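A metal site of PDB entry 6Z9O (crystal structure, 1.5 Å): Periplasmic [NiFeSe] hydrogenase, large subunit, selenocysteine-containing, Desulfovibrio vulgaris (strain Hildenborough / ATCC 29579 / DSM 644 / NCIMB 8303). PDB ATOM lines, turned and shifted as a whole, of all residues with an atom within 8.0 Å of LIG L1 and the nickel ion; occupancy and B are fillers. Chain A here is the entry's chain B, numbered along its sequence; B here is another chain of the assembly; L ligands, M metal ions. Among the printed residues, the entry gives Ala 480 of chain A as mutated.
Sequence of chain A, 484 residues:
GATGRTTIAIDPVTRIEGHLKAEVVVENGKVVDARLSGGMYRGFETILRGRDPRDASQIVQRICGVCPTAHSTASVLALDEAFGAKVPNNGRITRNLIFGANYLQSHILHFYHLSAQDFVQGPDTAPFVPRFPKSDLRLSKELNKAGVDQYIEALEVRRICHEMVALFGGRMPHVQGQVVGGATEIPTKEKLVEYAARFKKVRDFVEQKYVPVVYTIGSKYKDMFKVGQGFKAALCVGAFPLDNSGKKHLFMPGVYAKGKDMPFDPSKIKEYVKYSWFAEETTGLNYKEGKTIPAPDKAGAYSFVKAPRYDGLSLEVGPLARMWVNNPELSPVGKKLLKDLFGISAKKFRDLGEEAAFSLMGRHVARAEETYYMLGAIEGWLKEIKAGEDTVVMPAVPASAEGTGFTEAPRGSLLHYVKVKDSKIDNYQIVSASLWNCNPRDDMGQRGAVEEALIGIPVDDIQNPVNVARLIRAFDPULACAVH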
ATOM      1  N   GLU A  17     -16.067  32.135   4.438  1.00  0.00           N
ATOM      2  CA  GLU A  17     -14.919  31.275   4.205  1.00  0.00           C
ATOM      3  C   GLU A  17     -14.836  30.977   2.711  1.00  0.00           C
ATOM      4  O   GLU A  17     -15.840  30.697   2.061  1.00  0.00           O
ATOM      5  CB  GLU A  17     -15.006  29.971   4.978  1.00  0.00           C
ATOM      6  CG  GLU A  17     -13.743  29.076   4.908  1.00  0.00           C
ATOM      7  CD  GLU A  17     -13.508  28.433   3.542  1.00  0.00           C
ATOM      8  OE1 GLU A  17     -14.503  28.118   2.838  1.00  0.00           O
ATOM      9  OE2 GLU A  17     -12.331  28.243   3.180  1.00  0.00           O
ATOM     10  N   ARG A  42     -10.170  21.917  -5.552  1.00  0.00           N
ATOM     11  CA  ARG A  42      -9.089  21.011  -5.165  1.00  0.00           C
ATOM     12  C   ARG A  42      -9.315  19.583  -5.618  1.00  0.00           C
ATOM     13  O   ARG A  42      -8.356  18.915  -6.017  1.00  0.00           O
ATOM     14  CB  ARG A  42      -8.904  21.066  -3.637  1.00  0.00           C
ATOM     15  CG  ARG A  42      -8.211  22.341  -3.191  1.00  0.00           C
ATOM     16  CD  ARG A  42      -8.322  22.547  -1.701  1.00  0.00           C
ATOM     17  NE  ARG A  42      -9.720  22.713  -1.307  1.00  0.00           N
ATOM     18  CZ  ARG A  42     -10.185  22.606  -0.069  1.00  0.00           C
ATOM     19  NH1 ARG A  42      -9.356  22.326   0.926  1.00  0.00           N
ATOM     20  NH2 ARG A  42     -11.482  22.760   0.167  1.00  0.00           N
ATOM     21  N   GLN A  61     -11.323  16.051   6.319  1.00  0.00           N
ATOM     22  CA  GLN A  61     -11.404  17.217   7.184  1.00  0.00           C
ATOM     23  C   GLN A  61     -10.741  18.416   6.535  1.00  0.00           C
ATOM     24  O   GLN A  61     -11.157  19.559   6.766  1.00  0.00           O
ATOM     25  CB  GLN A  61     -10.770  16.939   8.540  1.00  0.00           C
ATOM     26  CG  GLN A  61     -11.559  15.955   9.360  1.00  0.00           C
ATOM     27  CD  GLN A  61     -11.087  15.903  10.784  1.00  0.00           C
ATOM     28  OE1 GLN A  61     -11.313  16.842  11.561  1.00  0.00           O
ATOM     29  NE2 GLN A  61     -10.417  14.824  11.142  1.00  0.00           N
ATOM     30  N   ILE A  63     -11.039  19.424   3.705  1.00  0.00           N
ATOM     31  CA  ILE A  63     -11.963  20.218   2.899  1.00  0.00           C
ATOM     32  C   ILE A  63     -12.150  21.591   3.515  1.00  0.00           C
ATOM     33  O   ILE A  63     -12.240  22.596   2.807  1.00  0.00           O
ATOM     34  CB  ILE A  63     -13.298  19.476   2.744  1.00  0.00           C
ATOM     35  CG1 ILE A  63     -13.116  18.250   1.853  1.00  0.00           C
ATOM     36  CG2 ILE A  63     -14.355  20.430   2.162  1.00  0.00           C
ATOM     37  CD1 ILE A  63     -14.272  17.298   1.862  1.00  0.00           C
ATOM     38  N   CYS A  64     -12.190  21.656   4.851  1.00  0.00           N
ATOM     39  CA  CYS A  64     -12.562  22.892   5.527  1.00  0.00           C
ATOM     40  C   CYS A  64     -12.055  22.866   6.946  1.00  0.00           C
ATOM     41  O   CYS A  64     -12.338  21.929   7.694  1.00  0.00           O
ATOM     42  CB  CYS A  64     -14.081  23.093   5.509  1.00  0.00           C
ATOM     43  SG  CYS A  64     -14.613  24.578   6.401  1.00  0.00           S
ATOM     44  N   GLY A  65     -11.312  23.900   7.324  1.00  0.00           N
ATOM     45  CA  GLY A  65     -10.806  24.030   8.674  1.00  0.00           C
ATOM     46  C   GLY A  65     -11.713  24.739   9.657  1.00  0.00           C
ATOM     47  O   GLY A  65     -11.384  24.823  10.836  1.00  0.00           O
ATOM     48  N   VAL A  66     -12.844  25.261   9.176  1.00  0.00           N
ATOM     49  CA  VAL A  66     -13.857  25.829  10.056  1.00  0.00           C
ATOM     50  C   VAL A  66     -14.841  24.760  10.526  1.00  0.00           C
ATOM     51  O   VAL A  66     -15.239  24.747  11.691  1.00  0.00           O
ATOM     52  CB  VAL A  66     -14.597  26.984   9.344  1.00  0.00           C
ATOM     53  CG1 VAL A  66     -15.670  27.566  10.253  1.00  0.00           C
ATOM     54  CG2 VAL A  66     -13.621  28.066   8.926  1.00  0.00           C
ATOM     55  N   CYS A  67     -15.205  23.824   9.633  1.00  0.00           N
ATOM     56  CA  CYS A  67     -16.150  22.760   9.944  1.00  0.00           C
ATOM     57  C   CYS A  67     -15.559  21.368   9.766  1.00  0.00           C
ATOM     58  O   CYS A  67     -16.247  20.457   9.282  1.00  0.00           O
ATOM     59  CB  CYS A  67     -17.403  22.883   9.067  1.00  0.00           C
ATOM     60  SG  CYS A  67     -17.097  22.546   7.304  1.00  0.00           S
ATOM     61  N   PRO A  68     -14.299  21.133  10.160  1.00  0.00           N
ATOM     62  CA  PRO A  68     -13.723  19.800   9.909  1.00  0.00           C
ATOM     63  C   PRO A  68     -14.421  18.695  10.669  1.00  0.00           C
ATOM     64  O   PRO A  68     -14.511  17.575  10.154  1.00  0.00           O
ATOM     65  CB  PRO A  68     -12.256  19.962  10.327  1.00  0.00           C
ATOM     66  CG  PRO A  68     -12.273  21.071  11.330  1.00  0.00           C
ATOM     67  CD  PRO A  68     -13.388  21.987  10.940  1.00  0.00           C
ATOM     68  N   ALA A  70     -17.504  18.275  11.088  1.00  0.00           N
ATOM     69  CA  ALA A  70     -18.653  17.816  10.318  1.00  0.00           C
ATOM     70  C   ALA A  70     -18.231  16.777   9.274  1.00  0.00           C
ATOM     71  O   ALA A  70     -18.875  15.735   9.134  1.00  0.00           O
ATOM     72  CB  ALA A  70     -19.338  19.009   9.639  1.00  0.00           C
ATOM     73  N   HIS A  71     -17.150  17.051   8.536  1.00  0.00           N
ATOM     74  CA  HIS A  71     -16.668  16.099   7.540  1.00  0.00           C
ATOM     75  C   HIS A  71     -16.121  14.843   8.212  1.00  0.00           C
ATOM     76  O   HIS A  71     -16.316  13.734   7.709  1.00  0.00           O
ATOM     77  CB  HIS A  71     -15.614  16.757   6.664  1.00  0.00           C
ATOM     78  CG  HIS A  71     -16.165  17.796   5.748  1.00  0.00           C
ATOM     79  ND1 HIS A  71     -16.933  17.478   4.643  1.00  0.00           N
ATOM     80  CD2 HIS A  71     -16.087  19.145   5.784  1.00  0.00           C
ATOM     81  CE1 HIS A  71     -17.297  18.592   4.027  1.00  0.00           C
ATOM     82  NE2 HIS A  71     -16.801  19.615   4.698  1.00  0.00           N
ATOM     83  N   ASN A 102     -18.070  22.161  18.379  1.00  0.00           N
ATOM     84  CA  ASN A 102     -17.743  23.012  17.245  1.00  0.00           C
ATOM     85  C   ASN A 102     -18.945  23.719  16.644  1.00  0.00           C
ATOM     86  O   ASN A 102     -18.765  24.701  15.931  1.00  0.00           O
ATOM     87  CB  ASN A 102     -17.025  22.252  16.136  1.00  0.00           C
ATOM     88  CG  ASN A 102     -16.231  23.189  15.241  1.00  0.00           C
ATOM     89  OD1 ASN A 102     -15.466  24.015  15.743  1.00  0.00           O
ATOM     90  ND2 ASN A 102     -16.432  23.107  13.932  1.00  0.00           N
ATOM     91  N   SER A 106     -18.508  27.512  15.768  1.00  0.00           N
ATOM     92  CA  SER A 106     -18.753  27.973  14.406  1.00  0.00           C
ATOM     93  C   SER A 106     -19.814  29.064  14.373  1.00  0.00           C
ATOM     94  O   SER A 106     -19.672  30.046  13.635  1.00  0.00           O
ATOM     95  CB  SER A 106     -19.170  26.796  13.529  1.00  0.00           C
ATOM     96  OG  SER A 106     -19.319  27.193  12.178  1.00  0.00           O
ATOM     97  N   LEU A 109     -18.248  32.202  15.937  1.00  0.00           N
ATOM     98  CA  LEU A 109     -17.354  32.749  14.924  1.00  0.00           C
ATOM     99  C   LEU A 109     -18.146  33.456  13.834  1.00  0.00           C
ATOM    100  O   LEU A 109     -17.798  34.564  13.395  1.00  0.00           O
ATOM    101  CB  LEU A 109     -16.497  31.640  14.312  1.00  0.00           C
ATOM    102  CG  LEU A 109     -15.620  32.019  13.107  1.00  0.00           C
ATOM    103  CD1 LEU A 109     -14.345  32.703  13.577  1.00  0.00           C
ATOM    104  CD2 LEU A 109     -15.306  30.795  12.235  1.00  0.00           C
ATOM    105  N   LEU A 114     -17.423  37.141  11.474  1.00  0.00           N
ATOM    106  CA  LEU A 114     -17.787  37.278  10.074  1.00  0.00           C
ATOM    107  C   LEU A 114     -18.929  38.265   9.870  1.00  0.00           C
ATOM    108  O   LEU A 114     -18.808  39.209   9.076  1.00  0.00           O
ATOM    109  CB  LEU A 114     -18.158  35.897   9.501  1.00  0.00           C
ATOM    110  CG  LEU A 114     -17.125  34.791   9.760  1.00  0.00           C
ATOM    111  CD1 LEU A 114     -17.596  33.424   9.262  1.00  0.00           C
ATOM    112  CD2 LEU A 114     -15.796  35.124   9.122  1.00  0.00           C
ATOM    113  N   ALA A 409     -23.770  19.681   9.185  1.00  0.00           N
ATOM    114  CA  ALA A 409     -22.702  20.593   9.520  1.00  0.00           C
ATOM    115  C   ALA A 409     -23.314  21.893  10.043  1.00  0.00           C
ATOM    116  O   ALA A 409     -24.495  22.150   9.831  1.00  0.00           O
ATOM    117  CB  ALA A 409     -21.829  20.870   8.294  1.00  0.00           C
ATOM    118  N   PRO A 410     -22.530  22.724  10.749  1.00  0.00           N
ATOM    119  CA  PRO A 410     -23.077  23.996  11.244  1.00  0.00           C
ATOM    120  C   PRO A 410     -23.784  24.812  10.188  1.00  0.00           C
ATOM    121  O   PRO A 410     -24.734  25.552  10.496  1.00  0.00           O
ATOM    122  CB  PRO A 410     -21.832  24.717  11.776  1.00  0.00           C
ATOM    123  CG  PRO A 410     -20.925  23.600  12.206  1.00  0.00           C
ATOM    124  CD  PRO A 410     -21.137  22.511  11.192  1.00  0.00           C
ATOM    125  N   ARG A 411     -23.374  24.686   8.923  1.00  0.00           N
ATOM    126  CA  ARG A 411     -23.958  25.449   7.838  1.00  0.00           C
ATOM    127  C   ARG A 411     -25.010  24.681   7.048  1.00  0.00           C
ATOM    128  O   ARG A 411     -25.678  25.268   6.201  1.00  0.00           O
ATOM    129  CB  ARG A 411     -22.842  25.922   6.888  1.00  0.00           C
ATOM    130  CG  ARG A 411     -21.983  26.987   7.529  1.00  0.00           C
ATOM    131  CD  ARG A 411     -20.573  27.093   7.000  1.00  0.00           C
ATOM    132  NE  ARG A 411     -19.923  28.104   7.807  1.00  0.00           N
ATOM    133  CZ  ARG A 411     -19.387  27.868   9.002  1.00  0.00           C
ATOM    134  NH1 ARG A 411     -19.358  26.638   9.493  1.00  0.00           N
ATOM    135  NH2 ARG A 411     -18.873  28.864   9.700  1.00  0.00           N
ATOM    136  N   SER A 432     -22.311  18.707   0.307  1.00  0.00           N
ATOM    137  CA  SER A 432     -22.072  19.451   1.523  1.00  0.00           C
ATOM    138  C   SER A 432     -23.072  20.607   1.689  1.00  0.00           C
ATOM    139  O   SER A 432     -23.898  20.888   0.812  1.00  0.00           O
ATOM    140  CB  SER A 432     -20.638  19.979   1.523  1.00  0.00           C
ATOM    141  OG  SER A 432     -20.477  20.880   0.448  1.00  0.00           O
ATOM    142  N   ALA A 433     -22.946  21.299   2.811  1.00  0.00           N
ATOM    143  CA  ALA A 433     -23.923  22.319   3.189  1.00  0.00           C
ATOM    144  C   ALA A 433     -23.901  23.499   2.228  1.00  0.00           C
ATOM    145  O   ALA A 433     -24.910  23.813   1.587  1.00  0.00           O
ATOM    146  CB  ALA A 433     -23.669  22.782   4.621  1.00  0.00           C
ATOM    147  N   SER A 434     -22.766  24.191   2.134  1.00  0.00           N
ATOM    148  CA  SER A 434     -22.720  25.372   1.282  1.00  0.00           C
ATOM    149  C   SER A 434     -22.814  25.024  -0.197  1.00  0.00           C
ATOM    150  O   SER A 434     -23.007  25.934  -1.010  1.00  0.00           O
ATOM    151  CB  SER A 434     -21.448  26.184   1.545  1.00  0.00           C
ATOM    152  OG  SER A 434     -21.474  26.745   2.847  1.00  0.00           O
ATOM    153  N   ASP A 476     -23.920  32.144   6.024  1.00  0.00           N
ATOM    154  CA  ASP A 476     -22.673  31.626   6.578  1.00  0.00           C
ATOM    155  C   ASP A 476     -21.931  30.774   5.560  1.00  0.00           C
ATOM    156  O   ASP A 476     -21.590  29.620   5.849  1.00  0.00           O
ATOM    157  CB  ASP A 476     -22.993  30.843   7.858  1.00  0.00           C
ATOM    158  CG  ASP A 476     -21.759  30.432   8.661  1.00  0.00           C
ATOM    159  OD1 ASP A 476     -20.613  30.859   8.372  1.00  0.00           O
ATOM    160  OD2 ASP A 476     -21.961  29.656   9.605  1.00  0.00           O
ATOM    161  N   PRO A 477     -21.655  31.297   4.357  1.00  0.00           N
ATOM    162  CA  PRO A 477     -21.064  30.459   3.320  1.00  0.00           C
ATOM    163  C   PRO A 477     -19.643  30.024   3.565  1.00  0.00           C
ATOM    164  O   PRO A 477     -18.844  30.740   4.165  1.00  0.00           O
ATOM    165  CB  PRO A 477     -21.080  31.351   2.068  1.00  0.00           C
ATOM    166  CG  PRO A 477     -21.888  32.528   2.401  1.00  0.00           C
ATOM    167  CD  PRO A 477     -21.836  32.682   3.887  1.00  0.00           C
ATOM    168  N   SEC A 478     -19.287  28.811   3.147  1.00  0.00           N
ATOM    169  CA  SEC A 478     -17.876  28.455   3.071  1.00  0.00           C
ATOM    170  CB  SEC A 478     -17.328  27.789   4.338  1.00  0.00           C
ATOM    171 SE   SEC A 478     -18.170  26.211   5.080  1.00  0.00          SE
ATOM    172  C   SEC A 478     -17.674  27.610   1.847  1.00  0.00           C
ATOM    173  O   SEC A 478     -18.035  26.434   1.791  1.00  0.00           O
ATOM    174  N   LEU A 479     -17.068  28.259   0.851  1.00  0.00           N
ATOM    175  CA  LEU A 479     -16.915  27.733  -0.502  1.00  0.00           C
ATOM    176  C   LEU A 479     -15.904  26.593  -0.584  1.00  0.00           C
ATOM    177  O   LEU A 479     -15.957  25.795  -1.512  1.00  0.00           O
ATOM    178  CB  LEU A 479     -16.540  28.866  -1.464  1.00  0.00           C
ATOM    179  CG  LEU A 479     -17.749  29.647  -2.000  1.00  0.00           C
ATOM    180  CD1 LEU A 479     -18.570  28.773  -2.966  1.00  0.00           C
ATOM    181  CD2 LEU A 479     -18.643  30.169  -0.884  1.00  0.00           C
ATOM    182  N   ALA A 480     -14.990  26.505   0.388  1.00  0.00           N
ATOM    183  CA  ALA A 480     -14.153  25.312   0.450  1.00  0.00           C
ATOM    184  C   ALA A 480     -15.011  24.062   0.571  1.00  0.00           C
ATOM    185  O   ALA A 480     -14.776  23.063  -0.125  1.00  0.00           O
ATOM    186  CB  ALA A 480     -13.167  25.411   1.615  1.00  0.00           C
ATOM    187  N   CYS A 481     -16.027  24.099   1.432  1.00  0.00           N
ATOM    188  CA  CYS A 481     -16.975  22.993   1.561  1.00  0.00           C
ATOM    189  C   CYS A 481     -17.798  22.815   0.302  1.00  0.00           C
ATOM    190  O   CYS A 481     -18.091  21.687  -0.103  1.00  0.00           O
ATOM    191  CB  CYS A 481     -17.920  23.234   2.730  1.00  0.00           C
ATOM    192  SG  CYS A 481     -17.262  22.785   4.305  1.00  0.00           S
ATOM    193  N   ALA A 482     -18.228  23.923  -0.311  1.00  0.00           N
ATOM    194  CA  ALA A 482     -19.143  23.831  -1.433  1.00  0.00           C
ATOM    195  C   ALA A 482     -18.481  23.145  -2.626  1.00  0.00           C
ATOM    196  O   ALA A 482     -19.150  22.409  -3.358  1.00  0.00           O
ATOM    197  CB  ALA A 482     -19.644  25.218  -1.822  1.00  0.00           C
ATOM    198  N   CYS B  18      -7.880  25.468   3.210  1.00  0.00           N
ATOM    199  CA  CYS B  18      -9.140  25.145   3.861  1.00  0.00           C
ATOM    200  C   CYS B  18      -9.487  26.135   4.970  1.00  0.00           C
ATOM    201  O   CYS B  18     -10.480  25.946   5.668  1.00  0.00           O
ATOM    202  CB  CYS B  18      -9.102  23.708   4.407  1.00  0.00           C
ATOM    203  SG  CYS B  18      -8.388  23.446   6.057  1.00  0.00           S
ATOM    204  N   THR B  19      -8.685  27.196   5.128  1.00  0.00           N
ATOM    205  CA  THR B  19      -8.854  28.234   6.152  1.00  0.00           C
ATOM    206  C   THR B  19      -8.478  27.730   7.535  1.00  0.00           C
ATOM    207  O   THR B  19      -8.571  28.472   8.521  1.00  0.00           O
ATOM    208  CB  THR B  19     -10.278  28.803   6.113  1.00  0.00           C
ATOM    209  OG1 THR B  19     -10.545  29.254   4.785  1.00  0.00           O
ATOM    210  CG2 THR B  19     -10.452  29.985   7.046  1.00  0.00           C
HETATM  211  S1  LIG L   1     -17.417  25.856   7.092  1.00  0.00           S
HETATM  212 FE1  LG2 L   2     -18.841  23.062   5.961  1.00  0.00          FE
HETATM  213  C1  LG2 L   2     -19.934  23.976   4.811  1.00  0.00           C
HETATM  214  N1  LG2 L   2     -20.649  24.554   4.114  1.00  0.00           N
HETATM  215  C2  LG2 L   2     -19.855  23.574   7.396  1.00  0.00           C
HETATM  216  N2  LG2 L   2     -20.492  23.896   8.304  1.00  0.00           N
HETATM  217  C3  LG2 L   2     -19.743  21.539   5.588  1.00  0.00           C
HETATM  218  O1  LG2 L   2     -20.341  20.616   5.331  1.00  0.00           O
HETATM  219  S1  LG3 L   3     -18.197  21.192  12.220  1.00  0.00           S
HETATM  220 NI    NI M   1     -16.840  24.382   5.849  1.00  0.00          NI
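A sulfur (S1) of LIG L1 is covalently linked to SE of SEC 478 (2.2 Å). The guanidinium group of Arg 411 lies close to a sulfur (S1) of LIG L1 (3.2 Å). An iron atom (FE1) of LG2 L2 is bound by the side-chain sulfur (SG) of Cys 481 (2.3 Å). An iron atom (FE1) of LG2 L2 is bound by the side-chain sulfur (SG) of Cys 67 (2.3 Å). The backbone NH (N) of Arg 411 sits at hydrogen-bond distance from a nitrogen (N2) of LG2 L2, at 3.1 Å. N2 of LG2 L2 sits at hydrogen-bond distance from NH1 of Arg 411, 3.2 Å away. The backbone NH of Ser 434 is in hydrogen-bond range of a nitrogen (N1) of LG2 L2 (2.9 Å). The side-chain hydroxyl (OG) of Ser 434 is in hydrogen-bond range of a nitrogen (N1) of LG2 L2 (2.7 Å). A sulfur (S1) of LG3 L3 lies close to the backbone carbonyl oxygen of Cys 67. The backbone NH (N) of Ala 70 sits close to a sulfur (S1) of LG3 L3 (3.2 Å). ND2 of Asn 102 sits close to S1 of LG3 L3, at 3.1 Å.
OG of Ser 434 lies within hydrogen-bond range of N of SEC 478 (3.0 Å). SG of Cys 481 sits close to NE2 of His 71, at 3.2 Å. O of Cys 481 sits at hydrogen-bond distance from OG of Ser 432, 2.6 Å away. The backbone NH of Val 66 lies close to the side-chain sulfur of Cys 64 (3.4 Å). NH1 of Arg 411 sits at hydrogen-bond distance from OG of Ser 106. NE of Arg 411 is in salt-bridge range of OD1 of Asp 476, 2.9 Å away. The backbone carbonyl oxygen of Val 66 lies within hydrogen-bond range of the side-chain amide nitrogen of Asn 102 (3.0 Å).
Val 66 touches LIG L1.
The nearest printed residue that does not touch the nickel ion is Arg 411 (4.8 Å).
The nickel ion is bound by S1 of LIG L1, SG of Cys 481, SG of Cys 64, SG of Cys 67 and SE of SEC 478. The nickel ion has five donor atoms within binding distance.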
